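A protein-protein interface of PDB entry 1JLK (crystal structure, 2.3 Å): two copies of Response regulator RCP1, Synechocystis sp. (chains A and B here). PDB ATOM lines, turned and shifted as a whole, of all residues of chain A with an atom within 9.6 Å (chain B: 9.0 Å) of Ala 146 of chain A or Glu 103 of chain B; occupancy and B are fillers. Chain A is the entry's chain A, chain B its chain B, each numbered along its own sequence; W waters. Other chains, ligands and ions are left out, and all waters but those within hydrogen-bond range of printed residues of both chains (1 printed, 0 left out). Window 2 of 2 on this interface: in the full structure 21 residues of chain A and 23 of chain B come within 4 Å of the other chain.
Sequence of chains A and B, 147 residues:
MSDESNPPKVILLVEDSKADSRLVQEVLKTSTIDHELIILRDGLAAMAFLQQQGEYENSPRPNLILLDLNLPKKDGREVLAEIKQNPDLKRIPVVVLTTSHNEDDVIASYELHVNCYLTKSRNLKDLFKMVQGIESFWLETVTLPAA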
ATOM      1  N   PRO A   7      13.818  -7.527 -14.769  1.00  0.00           N
ATOM      2  CA  PRO A   7      14.553  -6.710 -13.799  1.00  0.00           C
ATOM      3  C   PRO A   7      15.164  -7.541 -12.666  1.00  0.00           C
ATOM      4  O   PRO A   7      14.562  -8.509 -12.198  1.00  0.00           O
ATOM      5  CB  PRO A   7      13.488  -5.742 -13.297  1.00  0.00           C
ATOM      6  CG  PRO A   7      12.258  -6.601 -13.306  1.00  0.00           C
ATOM      7  CD  PRO A   7      12.363  -7.332 -14.628  1.00  0.00           C
ATOM      8  N   LYS A   9      16.258  -9.059  -9.156  1.00  0.00           N
ATOM      9  CA  LYS A   9      15.531  -9.232  -7.902  1.00  0.00           C
ATOM     10  C   LYS A   9      16.346  -8.557  -6.803  1.00  0.00           C
ATOM     11  O   LYS A   9      17.521  -8.867  -6.626  1.00  0.00           O
ATOM     12  CB  LYS A   9      15.390 -10.717  -7.581  1.00  0.00           C
ATOM     13  CG  LYS A   9      14.601 -11.499  -8.617  1.00  0.00           C
ATOM     14  CD  LYS A   9      13.133 -11.109  -8.578  1.00  0.00           C
ATOM     15  CE  LYS A   9      12.342 -11.802  -9.670  1.00  0.00           C
ATOM     16  NZ  LYS A   9      10.917 -11.363  -9.644  1.00  0.00           N
ATOM     17  N   ARG A  61      14.013  -0.420  -4.583  1.00  0.00           N
ATOM     18  CA  ARG A  61      12.911  -1.010  -3.851  1.00  0.00           C
ATOM     19  C   ARG A  61      13.142  -2.519  -3.764  1.00  0.00           C
ATOM     20  O   ARG A  61      13.256  -3.196  -4.786  1.00  0.00           O
ATOM     21  CB  ARG A  61      11.591  -0.698  -4.563  1.00  0.00           C
ATOM     22  CG  ARG A  61      10.354  -1.063  -3.766  1.00  0.00           C
ATOM     23  CD  ARG A  61       9.190  -0.142  -4.119  1.00  0.00           C
ATOM     24  NE  ARG A  61       8.027  -0.355  -3.252  1.00  0.00           N
ATOM     25  CZ  ARG A  61       7.310  -1.473  -3.253  1.00  0.00           C
ATOM     26  NH1 ARG A  61       7.644  -2.456  -4.071  1.00  0.00           N
ATOM     27  NH2 ARG A  61       6.262  -1.608  -2.448  1.00  0.00           N
ATOM     28  N   PRO A  62      13.242  -3.062  -2.540  1.00  0.00           N
ATOM     29  CA  PRO A  62      13.459  -4.501  -2.383  1.00  0.00           C
ATOM     30  C   PRO A  62      12.219  -5.322  -2.752  1.00  0.00           C
ATOM     31  O   PRO A  62      11.090  -4.882  -2.542  1.00  0.00           O
ATOM     32  CB  PRO A  62      13.832  -4.630  -0.907  1.00  0.00           C
ATOM     33  CG  PRO A  62      13.049  -3.551  -0.263  1.00  0.00           C
ATOM     34  CD  PRO A  62      13.210  -2.388  -1.230  1.00  0.00           C
ATOM     35  N   ASN A  63      12.436  -6.505  -3.326  1.00  0.00           N
ATOM     36  CA  ASN A  63      11.335  -7.397  -3.703  1.00  0.00           C
ATOM     37  C   ASN A  63      11.117  -8.404  -2.571  1.00  0.00           C
ATOM     38  O   ASN A  63      10.069  -9.044  -2.470  1.00  0.00           O
ATOM     39  CB  ASN A  63      11.675  -8.156  -4.991  1.00  0.00           C
ATOM     40  CG  ASN A  63      11.939  -7.231  -6.167  1.00  0.00           C
ATOM     41  OD1 ASN A  63      13.054  -7.177  -6.691  1.00  0.00           O
ATOM     42  ND2 ASN A  63      10.914  -6.495  -6.587  1.00  0.00           N
ATOM     43  N   ASP A  88       3.209   2.325   1.522  1.00  0.00           N
ATOM     44  CA  ASP A  88       4.181   2.198   0.447  1.00  0.00           C
ATOM     45  C   ASP A  88       4.990   0.895   0.511  1.00  0.00           C
ATOM     46  O   ASP A  88       5.259   0.280  -0.521  1.00  0.00           O
ATOM     47  CB  ASP A  88       5.106   3.430   0.491  1.00  0.00           C
ATOM     48  CG  ASP A  88       6.228   3.372  -0.528  1.00  0.00           C
ATOM     49  OD1 ASP A  88       5.960   3.006  -1.693  1.00  0.00           O
ATOM     50  OD2 ASP A  88       7.376   3.710  -0.164  1.00  0.00           O
ATOM     51  N   LEU A  89       5.349   0.467   1.718  1.00  0.00           N
ATOM     52  CA  LEU A  89       6.157  -0.740   1.908  1.00  0.00           C
ATOM     53  C   LEU A  89       5.367  -2.009   2.210  1.00  0.00           C
ATOM     54  O   LEU A  89       5.859  -3.120   2.015  1.00  0.00           O
ATOM     55  CB  LEU A  89       7.150  -0.504   3.039  1.00  0.00           C
ATOM     56  CG  LEU A  89       8.023   0.741   2.887  1.00  0.00           C
ATOM     57  CD1 LEU A  89       8.816   0.965   4.162  1.00  0.00           C
ATOM     58  CD2 LEU A  89       8.955   0.568   1.691  1.00  0.00           C
ATOM     59  N   ARG A  91       3.147  -4.164   1.037  1.00  0.00           N
ATOM     60  CA  ARG A  91       3.120  -5.361   0.203  1.00  0.00           C
ATOM     61  C   ARG A  91       4.439  -6.135   0.043  1.00  0.00           C
ATOM     62  O   ARG A  91       4.430  -7.322  -0.284  1.00  0.00           O
ATOM     63  CB  ARG A  91       2.567  -4.987  -1.181  1.00  0.00           C
ATOM     64  CG  ARG A  91       3.474  -4.053  -1.964  1.00  0.00           C
ATOM     65  CD  ARG A  91       2.888  -3.648  -3.312  1.00  0.00           C
ATOM     66  NE  ARG A  91       1.701  -2.796  -3.193  1.00  0.00           N
ATOM     67  CZ  ARG A  91       1.235  -2.024  -4.178  1.00  0.00           C
ATOM     68  NH1 ARG A  91       1.852  -1.994  -5.355  1.00  0.00           N
ATOM     69  NH2 ARG A  91       0.156  -1.275  -3.987  1.00  0.00           N
ATOM     70  N   ILE A  92       5.569  -5.478   0.263  1.00  0.00           N
ATOM     71  CA  ILE A  92       6.861  -6.154   0.133  1.00  0.00           C
ATOM     72  C   ILE A  92       6.939  -7.322   1.116  1.00  0.00           C
ATOM     73  O   ILE A  92       6.900  -7.113   2.323  1.00  0.00           O
ATOM     74  CB  ILE A  92       8.036  -5.198   0.450  1.00  0.00           C
ATOM     75  CG1 ILE A  92       7.952  -3.956  -0.429  1.00  0.00           C
ATOM     76  CG2 ILE A  92       9.368  -5.906   0.210  1.00  0.00           C
ATOM     77  CD1 ILE A  92       9.003  -2.916  -0.088  1.00  0.00           C
ATOM     78  N   PRO A  93       7.053  -8.567   0.613  1.00  0.00           N
ATOM     79  CA  PRO A  93       7.135  -9.728   1.507  1.00  0.00           C
ATOM     80  C   PRO A  93       8.288  -9.593   2.506  1.00  0.00           C
ATOM     81  O   PRO A  93       9.389  -9.176   2.142  1.00  0.00           O
ATOM     82  CB  PRO A  93       7.366 -10.893   0.541  1.00  0.00           C
ATOM     83  CG  PRO A  93       6.664 -10.445  -0.699  1.00  0.00           C
ATOM     84  CD  PRO A  93       7.089  -9.000  -0.799  1.00  0.00           C
ATOM     85  N   THR A 143       4.880 -15.513  -6.977  1.00  0.00           N
ATOM     86  CA  THR A 143       4.541 -14.425  -7.885  1.00  0.00           C
ATOM     87  C   THR A 143       4.633 -13.183  -6.993  1.00  0.00           C
ATOM     88  O   THR A 143       3.742 -12.937  -6.172  1.00  0.00           O
ATOM     89  CB  THR A 143       3.090 -14.556  -8.418  1.00  0.00           C
ATOM     90  OG1 THR A 143       3.036 -15.584  -9.409  1.00  0.00           O
ATOM     91  CG2 THR A 143       2.614 -13.245  -9.040  1.00  0.00           C
ATOM     92  N   LEU A 144       5.719 -12.422  -7.131  1.00  0.00           N
ATOM     93  CA  LEU A 144       5.916 -11.231  -6.309  1.00  0.00           C
ATOM     94  C   LEU A 144       5.125 -10.046  -6.826  1.00  0.00           C
ATOM     95  O   LEU A 144       4.818  -9.964  -8.019  1.00  0.00           O
ATOM     96  CB  LEU A 144       7.395 -10.870  -6.227  1.00  0.00           C
ATOM     97  CG  LEU A 144       8.248 -11.886  -5.475  1.00  0.00           C
ATOM     98  CD1 LEU A 144       9.691 -11.435  -5.474  1.00  0.00           C
ATOM     99  CD2 LEU A 144       7.728 -12.033  -4.060  1.00  0.00           C
ATOM    100  N   PRO A 145       4.773  -9.109  -5.931  1.00  0.00           N
ATOM    101  CA  PRO A 145       4.002  -7.938  -6.352  1.00  0.00           C
ATOM    102  C   PRO A 145       4.857  -6.779  -6.834  1.00  0.00           C
ATOM    103  O   PRO A 145       5.974  -6.557  -6.343  1.00  0.00           O
ATOM    104  CB  PRO A 145       3.233  -7.579  -5.092  1.00  0.00           C
ATOM    105  CG  PRO A 145       4.277  -7.831  -4.021  1.00  0.00           C
ATOM    106  CD  PRO A 145       4.917  -9.150  -4.461  1.00  0.00           C
ATOM    107  N   ALA A 146       4.315  -6.037  -7.796  1.00  0.00           N
ATOM    108  CA  ALA A 146       4.988  -4.864  -8.335  1.00  0.00           C
ATOM    109  C   ALA A 146       4.978  -3.785  -7.250  1.00  0.00           C
ATOM    110  O   ALA A 146       6.024  -3.115  -7.062  1.00  0.00           O
ATOM    111  CB  ALA A 146       4.264  -4.364  -9.586  1.00  0.00           C
ATOM    112  N   LEU B  69      -8.270 -18.206  -5.461  1.00  0.00           N
ATOM    113  CA  LEU B  69      -9.146 -17.041  -5.489  1.00  0.00           C
ATOM    114  C   LEU B  69     -10.493 -17.297  -6.180  1.00  0.00           C
ATOM    115  O   LEU B  69     -11.509 -16.717  -5.804  1.00  0.00           O
ATOM    116  CB  LEU B  69      -8.445 -15.872  -6.181  1.00  0.00           C
ATOM    117  CG  LEU B  69      -7.371 -15.116  -5.408  1.00  0.00           C
ATOM    118  CD1 LEU B  69      -6.922 -13.951  -6.255  1.00  0.00           C
ATOM    119  CD2 LEU B  69      -7.927 -14.614  -4.061  1.00  0.00           C
ATOM    120  N   SER B 100      -5.844 -17.473 -11.605  1.00  0.00           N
ATOM    121  CA  SER B 100      -5.878 -16.059 -11.981  1.00  0.00           C
ATOM    122  C   SER B 100      -4.523 -15.362 -12.175  1.00  0.00           C
ATOM    123  O   SER B 100      -3.793 -15.139 -11.211  1.00  0.00           O
ATOM    124  CB  SER B 100      -6.705 -15.281 -10.948  1.00  0.00           C
ATOM    125  OG  SER B 100      -6.597 -13.878 -11.152  1.00  0.00           O
ATOM    126  N   HIS B 101      -4.210 -15.003 -13.422  1.00  0.00           N
ATOM    127  CA  HIS B 101      -2.961 -14.303 -13.758  1.00  0.00           C
ATOM    128  C   HIS B 101      -3.152 -12.779 -13.720  1.00  0.00           C
ATOM    129  O   HIS B 101      -2.208 -12.027 -13.939  1.00  0.00           O
ATOM    130  CB  HIS B 101      -2.474 -14.680 -15.168  1.00  0.00           C
ATOM    131  CG  HIS B 101      -1.999 -16.095 -15.304  1.00  0.00           C
ATOM    132  ND1 HIS B 101      -2.860 -17.171 -15.356  1.00  0.00           N
ATOM    133  CD2 HIS B 101      -0.749 -16.609 -15.414  1.00  0.00           C
ATOM    134  CE1 HIS B 101      -2.161 -18.286 -15.493  1.00  0.00           C
ATOM    135  NE2 HIS B 101      -0.878 -17.972 -15.531  1.00  0.00           N
ATOM    136  N   ASN B 102      -4.375 -12.332 -13.450  1.00  0.00           N
ATOM    137  CA  ASN B 102      -4.705 -10.909 -13.409  1.00  0.00           C
ATOM    138  C   ASN B 102      -3.874 -10.084 -12.418  1.00  0.00           C
ATOM    139  O   ASN B 102      -3.797 -10.403 -11.227  1.00  0.00           O
ATOM    140  CB  ASN B 102      -6.204 -10.750 -13.117  1.00  0.00           C
ATOM    141  CG  ASN B 102      -6.598  -9.325 -12.817  1.00  0.00           C
ATOM    142  OD1 ASN B 102      -6.430  -8.848 -11.696  1.00  0.00           O
ATOM    143  ND2 ASN B 102      -7.128  -8.629 -13.823  1.00  0.00           N
ATOM    144  N   GLU B 103      -3.274  -9.010 -12.931  1.00  0.00           N
ATOM    145  CA  GLU B 103      -2.425  -8.109 -12.149  1.00  0.00           C
ATOM    146  C   GLU B 103      -3.137  -7.429 -10.985  1.00  0.00           C
ATOM    147  O   GLU B 103      -2.538  -7.205  -9.936  1.00  0.00           O
ATOM    148  CB  GLU B 103      -1.809  -7.042 -13.059  1.00  0.00           C
ATOM    149  CG  GLU B 103      -0.873  -6.076 -12.337  1.00  0.00           C
ATOM    150  CD  GLU B 103       0.361  -6.766 -11.784  1.00  0.00           C
ATOM    151  OE1 GLU B 103       1.096  -6.137 -10.989  1.00  0.00           O
ATOM    152  OE2 GLU B 103       0.600  -7.940 -12.148  1.00  0.00           O
ATOM    153  N   ASP B 104      -4.404  -7.079 -11.169  1.00  0.00           N
ATOM    154  CA  ASP B 104      -5.163  -6.452 -10.093  1.00  0.00           C
ATOM    155  C   ASP B 104      -5.243  -7.410  -8.891  1.00  0.00           C
ATOM    156  O   ASP B 104      -5.056  -6.998  -7.742  1.00  0.00           O
ATOM    157  CB  ASP B 104      -6.578  -6.104 -10.561  1.00  0.00           C
ATOM    158  CG  ASP B 104      -6.592  -5.091 -11.687  1.00  0.00           C
ATOM    159  OD1 ASP B 104      -6.039  -3.980 -11.504  1.00  0.00           O
ATOM    160  OD2 ASP B 104      -7.163  -5.408 -12.755  1.00  0.00           O
ATOM    161  N   ASP B 105      -5.521  -8.683  -9.163  1.00  0.00           N
ATOM    162  CA  ASP B 105      -5.616  -9.680  -8.102  1.00  0.00           C
ATOM    163  C   ASP B 105      -4.315  -9.832  -7.327  1.00  0.00           C
ATOM    164  O   ASP B 105      -4.332  -9.891  -6.104  1.00  0.00           O
ATOM    165  CB  ASP B 105      -6.025 -11.044  -8.660  1.00  0.00           C
ATOM    166  CG  ASP B 105      -7.445 -11.060  -9.169  1.00  0.00           C
ATOM    167  OD1 ASP B 105      -8.283 -10.326  -8.607  1.00  0.00           O
ATOM    168  OD2 ASP B 105      -7.730 -11.819 -10.120  1.00  0.00           O
ATOM    169  N   VAL B 106      -3.187  -9.887  -8.025  1.00  0.00           N
ATOM    170  CA  VAL B 106      -1.903 -10.040  -7.342  1.00  0.00           C
ATOM    171  C   VAL B 106      -1.684  -8.916  -6.331  1.00  0.00           C
ATOM    172  O   VAL B 106      -1.414  -9.162  -5.157  1.00  0.00           O
ATOM    173  CB  VAL B 106      -0.728 -10.044  -8.343  1.00  0.00           C
ATOM    174  CG1 VAL B 106       0.591 -10.184  -7.595  1.00  0.00           C
ATOM    175  CG2 VAL B 106      -0.891 -11.184  -9.347  1.00  0.00           C
ATOM    176  N   ILE B 107      -1.797  -7.677  -6.794  1.00  0.00           N
ATOM    177  CA  ILE B 107      -1.610  -6.510  -5.935  1.00  0.00           C
ATOM    178  C   ILE B 107      -2.636  -6.475  -4.798  1.00  0.00           C
ATOM    179  O   ILE B 107      -2.273  -6.481  -3.622  1.00  0.00           O
ATOM    180  CB  ILE B 107      -1.692  -5.214  -6.777  1.00  0.00           C
ATOM    181  CG1 ILE B 107      -0.512  -5.192  -7.763  1.00  0.00           C
ATOM    182  CG2 ILE B 107      -1.677  -3.978  -5.869  1.00  0.00           C
ATOM    183  CD1 ILE B 107      -0.616  -4.150  -8.848  1.00  0.00           C
ATOM    184  N   ALA B 108      -3.915  -6.453  -5.145  1.00  0.00           N
ATOM    185  CA  ALA B 108      -4.964  -6.433  -4.133  1.00  0.00           C
ATOM    186  C   ALA B 108      -4.780  -7.513  -3.050  1.00  0.00           C
ATOM    187  O   ALA B 108      -5.061  -7.270  -1.878  1.00  0.00           O
ATOM    188  CB  ALA B 108      -6.340  -6.597  -4.804  1.00  0.00           C
ATOM    189  N   SER B 109      -4.310  -8.699  -3.433  1.00  0.00           N
ATOM    190  CA  SER B 109      -4.128  -9.770  -2.453  1.00  0.00           C
ATOM    191  C   SER B 109      -3.002  -9.482  -1.479  1.00  0.00           C
ATOM    192  O   SER B 109      -3.141  -9.726  -0.284  1.00  0.00           O
ATOM    193  CB  SER B 109      -3.866 -11.113  -3.138  1.00  0.00           C
ATOM    194  OG  SER B 109      -5.023 -11.547  -3.823  1.00  0.00           O
ATOM    195  N   TYR B 110      -1.886  -8.965  -1.981  1.00  0.00           N
ATOM    196  CA  TYR B 110      -0.765  -8.657  -1.103  1.00  0.00           C
ATOM    197  C   TYR B 110      -1.117  -7.480  -0.206  1.00  0.00           C
ATOM    198  O   TYR B 110      -0.713  -7.434   0.950  1.00  0.00           O
ATOM    199  CB  TYR B 110       0.495  -8.360  -1.912  1.00  0.00           C
ATOM    200  CG  TYR B 110       1.254  -9.605  -2.328  1.00  0.00           C
ATOM    201  CD1 TYR B 110       1.247 -10.048  -3.648  1.00  0.00           C
ATOM    202  CD2 TYR B 110       2.001 -10.330  -1.398  1.00  0.00           C
ATOM    203  CE1 TYR B 110       1.969 -11.180  -4.033  1.00  0.00           C
ATOM    204  CE2 TYR B 110       2.722 -11.460  -1.774  1.00  0.00           C
ATOM    205  CZ  TYR B 110       2.701 -11.878  -3.090  1.00  0.00           C
ATOM    206  OH  TYR B 110       3.407 -13.009  -3.460  1.00  0.00           O
ATOM    207  N   GLU B 111      -1.900  -6.546  -0.736  1.00  0.00           N
ATOM    208  CA  GLU B 111      -2.313  -5.388   0.041  1.00  0.00           C
ATOM    209  C   GLU B 111      -3.262  -5.848   1.147  1.00  0.00           C
ATOM    210  O   GLU B 111      -3.335  -5.228   2.207  1.00  0.00           O
ATOM    211  CB  GLU B 111      -3.009  -4.355  -0.849  1.00  0.00           C
ATOM    212  CG  GLU B 111      -2.715  -2.919  -0.443  1.00  0.00           C
ATOM    213  CD  GLU B 111      -1.338  -2.456  -0.894  1.00  0.00           C
ATOM    214  OE1 GLU B 111      -1.190  -2.098  -2.081  1.00  0.00           O
ATOM    215  OE2 GLU B 111      -0.400  -2.457  -0.068  1.00  0.00           O
ATOM    216  N   TYR B 117       1.517 -15.281  -3.016  1.00  0.00           N
ATOM    217  CA  TYR B 117       0.582 -15.538  -4.097  1.00  0.00           C
ATOM    218  C   TYR B 117       1.291 -16.408  -5.127  1.00  0.00           C
ATOM    219  O   TYR B 117       2.401 -16.084  -5.569  1.00  0.00           O
ATOM    220  CB  TYR B 117       0.167 -14.182  -4.673  1.00  0.00           C
ATOM    221  CG  TYR B 117      -0.932 -14.168  -5.704  1.00  0.00           C
ATOM    222  CD1 TYR B 117      -2.130 -13.488  -5.451  1.00  0.00           C
ATOM    223  CD2 TYR B 117      -0.760 -14.757  -6.963  1.00  0.00           C
ATOM    224  CE1 TYR B 117      -3.121 -13.384  -6.425  1.00  0.00           C
ATOM    225  CE2 TYR B 117      -1.760 -14.660  -7.942  1.00  0.00           C
ATOM    226  CZ  TYR B 117      -2.932 -13.965  -7.659  1.00  0.00           C
ATOM    227  OH  TYR B 117      -3.914 -13.815  -8.622  1.00  0.00           O
ATOM    228  N   THR B 119       0.784 -18.725  -8.816  1.00  0.00           N
ATOM    229  CA  THR B 119      -0.036 -18.944 -10.001  1.00  0.00           C
ATOM    230  C   THR B 119       0.140 -20.363 -10.533  1.00  0.00           C
ATOM    231  O   THR B 119       1.256 -20.789 -10.828  1.00  0.00           O
ATOM    232  CB  THR B 119       0.315 -17.933 -11.114  1.00  0.00           C
ATOM    233  OG1 THR B 119      -0.151 -16.637 -10.730  1.00  0.00           O
ATOM    234  CG2 THR B 119      -0.341 -18.331 -12.441  1.00  0.00           C
HETATM  235  O   HOH W   1       3.761 -18.109  -8.979  1.00  0.00           O
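Hydrophobic or aromatic side chains of chain B within 4 Å of the printed part of chain A: Val 106, Ile 107 and Tyr 110.
Hydrophobic or aromatic side chains of chain A that line the printed part of chain B: Pro 145 and Ala 146.
Among the printed residues, 8 pairs touch across the chains.
Water W1 bridges OG1 of Thr 143 of chain A (2.7 Å) and N of Thr 119 of chain B (3.0 Å).
The guanidinium group (NH1) of Arg 61 of chain A sits at hydrogen-bond distance from the backbone carbonyl oxygen (O) of Ala 146 of chain A, 3.5 Å away.
The backbone carbonyl oxygen (O) of Ser 100 of chain B lies within hydrogen-bond range of the side-chain hydroxyl (OH) of Tyr 117 of chain B (2.9 Å).
N of Tyr 117 of chain B lies within hydrogen-bond range of OH of Tyr 110 of chain B, 3.0 Å away.
Of the printed residues of chain B, Thr 143 of chain A touches Val 106 (3.9 Å), Tyr 110 (2.7 Å), Tyr 117 (2.9 Å) and Thr 119 (3.6 Å).
Of chain B, only Glu 103 comes within 4 Å of Ala 146 of chain A.
Of chain A, only Ala 146 (3.9 Å) comes within 4 Å of Glu 103 of chain B.
No residue of chain A comes within 4 Å of Asp 104 of chain B.
Of chain A, only Thr 143 (3.9 Å) comes within 4 Å of Val 106 of chain B.
Printed residues of chain A within 4 Å of Ile 107 of chain B: Arg 91.
Of the printed residues of chain A, Glu 111 of chain B touches Arg 91.
Of the printed residues of chain A, Thr 119 of chain B touches Thr 143 (3.6 Å).
Arg 91 of chain A touches Ile 107 of chain B (NH2 to CG2, 3.8 Å).
Val 106 of chain B touches Thr 143 of chain A.
Thr 143 of chain A touches Thr 119 of chain B (OG1 to OG1, 3.6 Å).
Tyr 110 of chain B touches Pro 145 of chain A.
OE1 of Glu 103 of chain B touches CB of Ala 146 of chain A, at 3.9 Å.
No position is printed for both chains.
Of the 8 pairs that touch across the chains among the printed residues, none has its exchanged pair printed and touching as well.
O of Tyr 117 of chain B lies within hydrogen-bond range of N of Thr 143 of chain A (2.9 Å).
The guanidinium group (NH2) of Arg 91 of chain A is in salt-bridge range of the side-chain carboxylate (OE1) of Glu 111 of chain B (2.5 Å).
The side-chain hydroxyl (OH) of Tyr 110 of chain B lies within hydrogen-bond range of the backbone carbonyl oxygen (O) of Thr 143 of chain A, at 2.7 Å.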
